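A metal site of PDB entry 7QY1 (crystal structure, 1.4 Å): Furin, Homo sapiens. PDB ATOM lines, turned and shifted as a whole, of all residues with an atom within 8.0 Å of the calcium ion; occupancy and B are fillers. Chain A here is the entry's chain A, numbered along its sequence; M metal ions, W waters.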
ATOM      1  N   GLY A 148       8.445  31.949  21.384  1.00  0.00           N
ATOM      2  CA  GLY A 148       9.364  31.431  22.376  1.00  0.00           C
ATOM      3  C   GLY A 148      10.603  32.290  22.455  1.00  0.00           C
ATOM      4  O   GLY A 148      10.553  33.510  22.254  1.00  0.00           O
ATOM      5  N   PRO A 149      11.737  31.671  22.756  1.00  0.00           N
ATOM      6  CA  PRO A 149      13.001  32.424  22.731  1.00  0.00           C
ATOM      7  C   PRO A 149      13.272  32.990  21.343  1.00  0.00           C
ATOM      8  O   PRO A 149      12.736  32.533  20.338  1.00  0.00           O
ATOM      9  CB  PRO A 149      14.058  31.367  23.089  1.00  0.00           C
ATOM     10  CG  PRO A 149      13.354  30.218  23.504  1.00  0.00           C
ATOM     11  CD  PRO A 149      11.959  30.245  22.998  1.00  0.00           C
ATOM     12  N   GLU A 150      14.137  34.000  21.302  1.00  0.00           N
ATOM     13  CA  GLU A 150      14.374  34.731  20.067  1.00  0.00           C
ATOM     14  C   GLU A 150      14.794  33.795  18.940  1.00  0.00           C
ATOM     15  O   GLU A 150      15.655  32.929  19.111  1.00  0.00           O
ATOM     16  CB  GLU A 150      15.474  35.760  20.265  1.00  0.00           C
ATOM     17  CG  GLU A 150      15.054  36.932  21.100  1.00  0.00           C
ATOM     18  CD  GLU A 150      14.517  38.054  20.261  1.00  0.00           C
ATOM     19  OE1 GLU A 150      14.665  39.195  20.719  1.00  0.00           O
ATOM     20  OE2 GLU A 150      13.970  37.803  19.166  1.00  0.00           O
ATOM     21  N   ASP A 151      14.192  34.005  17.771  1.00  0.00           N
ATOM     22  CA  ASP A 151      14.479  33.227  16.563  1.00  0.00           C
ATOM     23  C   ASP A 151      15.623  33.869  15.771  1.00  0.00           C
ATOM     24  O   ASP A 151      15.540  34.092  14.559  1.00  0.00           O
ATOM     25  CB  ASP A 151      13.203  33.102  15.730  1.00  0.00           C
ATOM     26  CG  ASP A 151      12.195  32.102  16.301  1.00  0.00           C
ATOM     27  OD1 ASP A 151      12.607  31.170  17.037  1.00  0.00           O
ATOM     28  OD2 ASP A 151      10.977  32.203  15.964  1.00  0.00           O
ATOM     29  N   ASP A 152      16.719  34.163  16.479  1.00  0.00           N
ATOM     30  CA  ASP A 152      17.869  34.817  15.870  1.00  0.00           C
ATOM     31  C   ASP A 152      18.928  33.845  15.364  1.00  0.00           C
ATOM     32  O   ASP A 152      19.904  34.271  14.761  1.00  0.00           O
ATOM     33  CB  ASP A 152      18.478  35.862  16.836  1.00  0.00           C
ATOM     34  CG  ASP A 152      18.910  35.293  18.173  1.00  0.00           C
ATOM     35  OD1 ASP A 152      18.876  34.068  18.343  1.00  0.00           O
ATOM     36  OD2 ASP A 152      19.328  36.096  19.039  1.00  0.00           O
ATOM     37  N   GLY A 153      18.728  32.542  15.565  1.00  0.00           N
ATOM     38  CA  GLY A 153      19.707  31.574  15.115  1.00  0.00           C
ATOM     39  C   GLY A 153      20.949  31.518  15.969  1.00  0.00           C
ATOM     40  O   GLY A 153      21.932  30.894  15.568  1.00  0.00           O
ATOM     41  N   LYS A 154      20.930  32.163  17.140  1.00  0.00           N
ATOM     42  CA  LYS A 154      22.044  32.096  18.056  1.00  0.00           C
ATOM     43  C   LYS A 154      21.652  31.803  19.490  1.00  0.00           C
ATOM     44  O   LYS A 154      22.535  31.628  20.336  1.00  0.00           O
ATOM     45  CB  LYS A 154      22.912  33.362  18.001  1.00  0.00           C
ATOM     46  CG  LYS A 154      22.206  34.654  17.972  1.00  0.00           C
ATOM     47  CD  LYS A 154      23.205  35.768  17.598  1.00  0.00           C
ATOM     48  CE  LYS A 154      22.563  37.133  17.676  1.00  0.00           C
ATOM     49  N   THR A 155      20.373  31.671  19.788  1.00  0.00           N
ATOM     50  CA  THR A 155      19.929  31.483  21.165  1.00  0.00           C
ATOM     51  C   THR A 155      19.658  30.020  21.444  1.00  0.00           C
ATOM     52  O   THR A 155      19.100  29.299  20.609  1.00  0.00           O
ATOM     53  CB  THR A 155      18.625  32.278  21.346  1.00  0.00           C
ATOM     54  OG1 THR A 155      18.887  33.665  21.129  1.00  0.00           O
ATOM     55  CG2 THR A 155      18.068  32.119  22.741  1.00  0.00           C
ATOM     56  N   ALA A 185       4.237  26.476  18.061  1.00  0.00           N
ATOM     57  CA  ALA A 185       4.819  26.727  16.757  1.00  0.00           C
ATOM     58  C   ALA A 185       6.320  26.477  16.841  1.00  0.00           C
ATOM     59  O   ALA A 185       6.984  26.896  17.791  1.00  0.00           O
ATOM     60  CB  ALA A 185       4.599  28.200  16.380  1.00  0.00           C
ATOM     61  N   SER A 186       6.864  25.807  15.840  1.00  0.00           N
ATOM     62  CA  SER A 186       8.273  25.426  15.913  1.00  0.00           C
ATOM     63  C   SER A 186       9.243  26.574  15.637  1.00  0.00           C
ATOM     64  O   SER A 186      10.447  26.392  15.842  1.00  0.00           O
ATOM     65  CB  SER A 186       8.529  24.272  14.942  1.00  0.00           C
ATOM     66  OG  SER A 186       8.290  24.660  13.596  1.00  0.00           O
ATOM     67  N   GLY A 187       8.779  27.709  15.123  1.00  0.00           N
ATOM     68  CA  GLY A 187       9.602  28.895  15.047  1.00  0.00           C
ATOM     69  C   GLY A 187       9.559  29.558  13.682  1.00  0.00           C
ATOM     70  O   GLY A 187       9.136  28.980  12.680  1.00  0.00           O
ATOM     71  N   ASN A 188      10.048  30.808  13.666  1.00  0.00           N
ATOM     72  CA  ASN A 188      10.098  31.627  12.454  1.00  0.00           C
ATOM     73  C   ASN A 188      11.531  31.986  12.053  1.00  0.00           C
ATOM     74  O   ASN A 188      11.733  32.918  11.255  1.00  0.00           O
ATOM     75  CB  ASN A 188       9.300  32.935  12.615  1.00  0.00           C
ATOM     76  CG  ASN A 188       7.814  32.711  12.749  1.00  0.00           C
ATOM     77  OD1 ASN A 188       7.210  31.990  11.968  1.00  0.00           O
ATOM     78  ND2 ASN A 188       7.213  33.394  13.699  1.00  0.00           N
ATOM     79  N   GLY A 189      12.521  31.291  12.580  1.00  0.00           N
ATOM     80  CA  GLY A 189      13.917  31.646  12.360  1.00  0.00           C
ATOM     81  C   GLY A 189      14.615  31.142  11.118  1.00  0.00           C
ATOM     82  O   GLY A 189      15.851  31.115  11.086  1.00  0.00           O
ATOM     83  N   GLY A 190      13.864  30.733  10.097  1.00  0.00           N
ATOM     84  CA  GLY A 190      14.475  30.128   8.918  1.00  0.00           C
ATOM     85  C   GLY A 190      15.534  30.992   8.250  1.00  0.00           C
ATOM     86  O   GLY A 190      16.565  30.481   7.808  1.00  0.00           O
ATOM     87  N   HIS A 193      18.832  30.737   9.731  1.00  0.00           N
ATOM     88  CA  HIS A 193      19.318  29.352   9.805  1.00  0.00           C
ATOM     89  C   HIS A 193      19.146  28.788  11.199  1.00  0.00           C
ATOM     90  O   HIS A 193      19.974  28.005  11.688  1.00  0.00           O
ATOM     91  CB  HIS A 193      20.758  29.238   9.316  1.00  0.00           C
ATOM     92  CG  HIS A 193      20.951  29.865   7.990  1.00  0.00           C
ATOM     93  ND1 HIS A 193      20.386  29.345   6.852  1.00  0.00           N
ATOM     94  CD2 HIS A 193      21.563  31.013   7.610  1.00  0.00           C
ATOM     95  CE1 HIS A 193      20.685  30.115   5.810  1.00  0.00           C
ATOM     96  NE2 HIS A 193      21.389  31.136   6.252  1.00  0.00           N
ATOM     97  N   ASP A 194      18.056  29.155  11.857  1.00  0.00           N
ATOM     98  CA  ASP A 194      17.784  28.637  13.191  1.00  0.00           C
ATOM     99  C   ASP A 194      17.381  27.160  13.095  1.00  0.00           C
ATOM    100  O   ASP A 194      16.873  26.699  12.073  1.00  0.00           O
ATOM    101  CB  ASP A 194      16.710  29.501  13.855  1.00  0.00           C
ATOM    102  CG  ASP A 194      16.671  29.366  15.374  1.00  0.00           C
ATOM    103  OD1 ASP A 194      17.465  28.575  15.962  1.00  0.00           O
ATOM    104  OD2 ASP A 194      15.797  30.025  16.000  1.00  0.00           O
ATOM    105  N   SER A 195      17.658  26.425  14.165  1.00  0.00           N
ATOM    106  CA  SER A 195      17.494  24.965  14.250  1.00  0.00           C
ATOM    107  C   SER A 195      16.688  24.748  15.522  1.00  0.00           C
ATOM    108  O   SER A 195      17.155  25.059  16.606  1.00  0.00           O
ATOM    109  CB  SER A 195      18.889  24.336  14.316  1.00  0.00           C
ATOM    110  OG  SER A 195      18.882  22.915  14.188  1.00  0.00           O
ATOM    111  N   CYS A 196      15.443  24.266  15.398  1.00  0.00           N
ATOM    112  CA  CYS A 196      14.458  24.523  16.453  1.00  0.00           C
ATOM    113  C   CYS A 196      14.585  23.625  17.694  1.00  0.00           C
ATOM    114  O   CYS A 196      13.885  23.887  18.684  1.00  0.00           O
ATOM    115  CB  CYS A 196      13.020  24.526  15.932  1.00  0.00           C
ATOM    116  SG  CYS A 196      12.559  23.325  14.646  1.00  0.00           S
ATOM    117  N   ASN A 197      15.448  22.613  17.713  1.00  0.00           N
ATOM    118  CA  ASN A 197      15.639  21.944  19.009  1.00  0.00           C
ATOM    119  C   ASN A 197      16.342  22.850  20.017  1.00  0.00           C
ATOM    120  O   ASN A 197      16.398  22.509  21.211  1.00  0.00           O
ATOM    121  CB  ASN A 197      16.408  20.626  18.890  1.00  0.00           C
ATOM    122  CG  ASN A 197      15.651  19.561  18.141  1.00  0.00           C
ATOM    123  OD1 ASN A 197      14.421  19.582  17.961  1.00  0.00           O
ATOM    124  ND2 ASN A 197      16.404  18.551  17.714  1.00  0.00           N
ATOM    125  N   CYS A 198      16.873  24.006  19.581  1.00  0.00           N
ATOM    126  CA  CYS A 198      17.471  24.987  20.463  1.00  0.00           C
ATOM    127  C   CYS A 198      16.434  25.861  21.175  1.00  0.00           C
ATOM    128  O   CYS A 198      16.821  26.696  21.992  1.00  0.00           O
ATOM    129  CB  CYS A 198      18.439  25.887  19.683  1.00  0.00           C
ATOM    130  SG  CYS A 198      19.875  25.022  19.067  1.00  0.00           S
ATOM    131  N   ASP A 199      15.145  25.659  20.895  1.00  0.00           N
ATOM    132  CA  ASP A 199      14.004  26.275  21.566  1.00  0.00           C
ATOM    133  C   ASP A 199      13.401  25.196  22.451  1.00  0.00           C
ATOM    134  O   ASP A 199      12.808  24.232  21.957  1.00  0.00           O
ATOM    135  CB  ASP A 199      13.054  26.751  20.462  1.00  0.00           C
ATOM    136  CG  ASP A 199      11.665  27.187  20.951  1.00  0.00           C
ATOM    137  OD1 ASP A 199      11.243  26.890  22.101  1.00  0.00           O
ATOM    138  OD2 ASP A 199      10.972  27.808  20.099  1.00  0.00           O
ATOM    139  N   GLY A 200      13.585  25.341  23.762  1.00  0.00           N
ATOM    140  CA  GLY A 200      13.167  24.334  24.727  1.00  0.00           C
ATOM    141  C   GLY A 200      11.667  24.176  24.880  1.00  0.00           C
ATOM    142  O   GLY A 200      11.202  23.194  25.461  1.00  0.00           O
ATOM    143  N   THR A 202       9.369  24.308  22.063  1.00  0.00           N
ATOM    144  CA  THR A 202       8.995  23.388  20.998  1.00  0.00           C
ATOM    145  C   THR A 202       9.712  22.032  21.139  1.00  0.00           C
ATOM    146  O   THR A 202       9.138  21.005  20.797  1.00  0.00           O
ATOM    147  CB  THR A 202       9.209  24.054  19.647  1.00  0.00           C
ATOM    148  OG1 THR A 202       8.505  23.326  18.631  1.00  0.00           O
ATOM    149  CG2 THR A 202      10.686  24.160  19.278  1.00  0.00           C
ATOM    150  N   TYR A 222      10.621  31.074   6.329  1.00  0.00           N
ATOM    151  CA  TYR A 222      10.761  31.270   7.763  1.00  0.00           C
ATOM    152  C   TYR A 222      10.848  29.960   8.553  1.00  0.00           C
ATOM    153  O   TYR A 222      11.077  30.019   9.771  1.00  0.00           O
ATOM    154  CB  TYR A 222       9.584  32.129   8.299  1.00  0.00           C
ATOM    155  CG  TYR A 222       8.227  31.604   7.864  1.00  0.00           C
ATOM    156  CD1 TYR A 222       7.652  30.516   8.504  1.00  0.00           C
ATOM    157  CD2 TYR A 222       7.539  32.169   6.780  1.00  0.00           C
ATOM    158  CE1 TYR A 222       6.448  30.000   8.098  1.00  0.00           C
ATOM    159  CE2 TYR A 222       6.323  31.655   6.366  1.00  0.00           C
ATOM    160  CZ  TYR A 222       5.777  30.564   7.037  1.00  0.00           C
ATOM    161  OH  TYR A 222       4.580  29.993   6.690  1.00  0.00           O
ATOM    162  N   GLU A 224      11.896  26.583  10.468  1.00  0.00           N
ATOM    163  CA  GLU A 224      13.043  25.957  11.105  1.00  0.00           C
ATOM    164  C   GLU A 224      12.847  24.454  11.052  1.00  0.00           C
ATOM    165  O   GLU A 224      11.763  23.957  11.386  1.00  0.00           O
ATOM    166  CB  GLU A 224      13.156  26.385  12.567  1.00  0.00           C
ATOM    167  CG  GLU A 224      13.286  27.892  12.756  1.00  0.00           C
ATOM    168  CD  GLU A 224      13.405  28.327  14.222  1.00  0.00           C
ATOM    169  OE1 GLU A 224      14.044  27.612  15.037  1.00  0.00           O
ATOM    170  OE2 GLU A 224      12.892  29.412  14.572  1.00  0.00           O
ATOM    171  N   CYS A 226      13.769  20.749  12.582  1.00  0.00           N
ATOM    172  CA  CYS A 226      14.316  20.068  13.742  1.00  0.00           C
ATOM    173  C   CYS A 226      13.575  18.755  13.970  1.00  0.00           C
ATOM    174  O   CYS A 226      12.460  18.547  13.469  1.00  0.00           O
ATOM    175  CB  CYS A 226      14.286  20.930  15.015  1.00  0.00           C
ATOM    176  SG  CYS A 226      12.692  21.521  15.556  1.00  0.00           S
ATOM    177  N   ARG A 412      24.465  26.276  12.904  1.00  0.00           N
ATOM    178  CA  ARG A 412      23.837  27.598  13.031  1.00  0.00           C
ATOM    179  C   ARG A 412      24.926  28.655  12.856  1.00  0.00           C
ATOM    180  O   ARG A 412      25.658  28.965  13.815  1.00  0.00           O
ATOM    181  CB  ARG A 412      23.137  27.741  14.382  1.00  0.00           C
ATOM    182  CG  ARG A 412      21.910  26.843  14.533  1.00  0.00           C
ATOM    183  CD  ARG A 412      20.916  27.343  15.590  1.00  0.00           C
ATOM    184  NE  ARG A 412      21.556  27.559  16.896  1.00  0.00           N
ATOM    185  CZ  ARG A 412      20.995  28.232  17.897  1.00  0.00           C
ATOM    186  NH1 ARG A 412      19.778  28.758  17.767  1.00  0.00           N
ATOM    187  NH2 ARG A 412      21.666  28.397  19.024  1.00  0.00           N
HETATM  188 CA    CA M   1      13.815  29.183  16.872  1.00  0.00          CA
HETATM  189  O   HOH W   1      15.498  27.700  17.897  1.00  0.00           O
HETATM  190  O   HOH W   2      14.175  30.085  19.135  1.00  0.00           O
HETATM  191  O   HOH W   3      11.983  27.855  17.607  1.00  0.00           O
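N of Asp 194 is in hydrogen-bond range of O of Gly 189 (3.0 Å). The side-chain carboxylate (OE2) of Glu 224 lies close to the backbone NH (N) of Gly 189, 2.8 Å away. The backbone NH (N) of Asn 188 lies close to the side-chain carboxylate (OE2) of Glu 224 (3.3 Å). The side-chain carboxylate (OD2) of Asp 151 is in hydrogen-bond range of the backbone NH (N) of Asn 188, at 2.8 Å. The side-chain sulfur (SG) of Cys 196 forms a disulfide with the side-chain sulfur (SG) of Cys 226, 2.0 Å away. The side-chain carboxylate (OD1) of Asp 194 lies within salt-bridge range of the guanidinium group (NH1) of Arg 412, 2.9 Å away.
Three residues have an atom within 4 Å of the calcium ion: Asp 151, Asp 194 and Glu 224. Along chain A the residues within 4 Å of the calcium ion span positions 151 to 224. The nearest printed residue that does not touch the calcium ion is Asp 199 (4.4 Å).
The calcium ion is bound by OD2 of Asp 194 (2.3 Å), OD1 of Asp 151 (2.3 Å), water W3 (2.4 Å), OE1 of Glu 224 (2.4 Å), water W2 (2.5 Å), water W1 (2.5 Å) and OE2 of Glu 224 (2.5 Å).
Water W3 lies within hydrogen-bond range of OD2 of Asp 199 (2.7 Å) and O of Ser 186 (2.8 Å). Water W1 bridges the side-chain carboxylate of Asp 194 (2.9 Å) and the backbone carbonyl oxygen of Ser 195 (3.4 Å).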
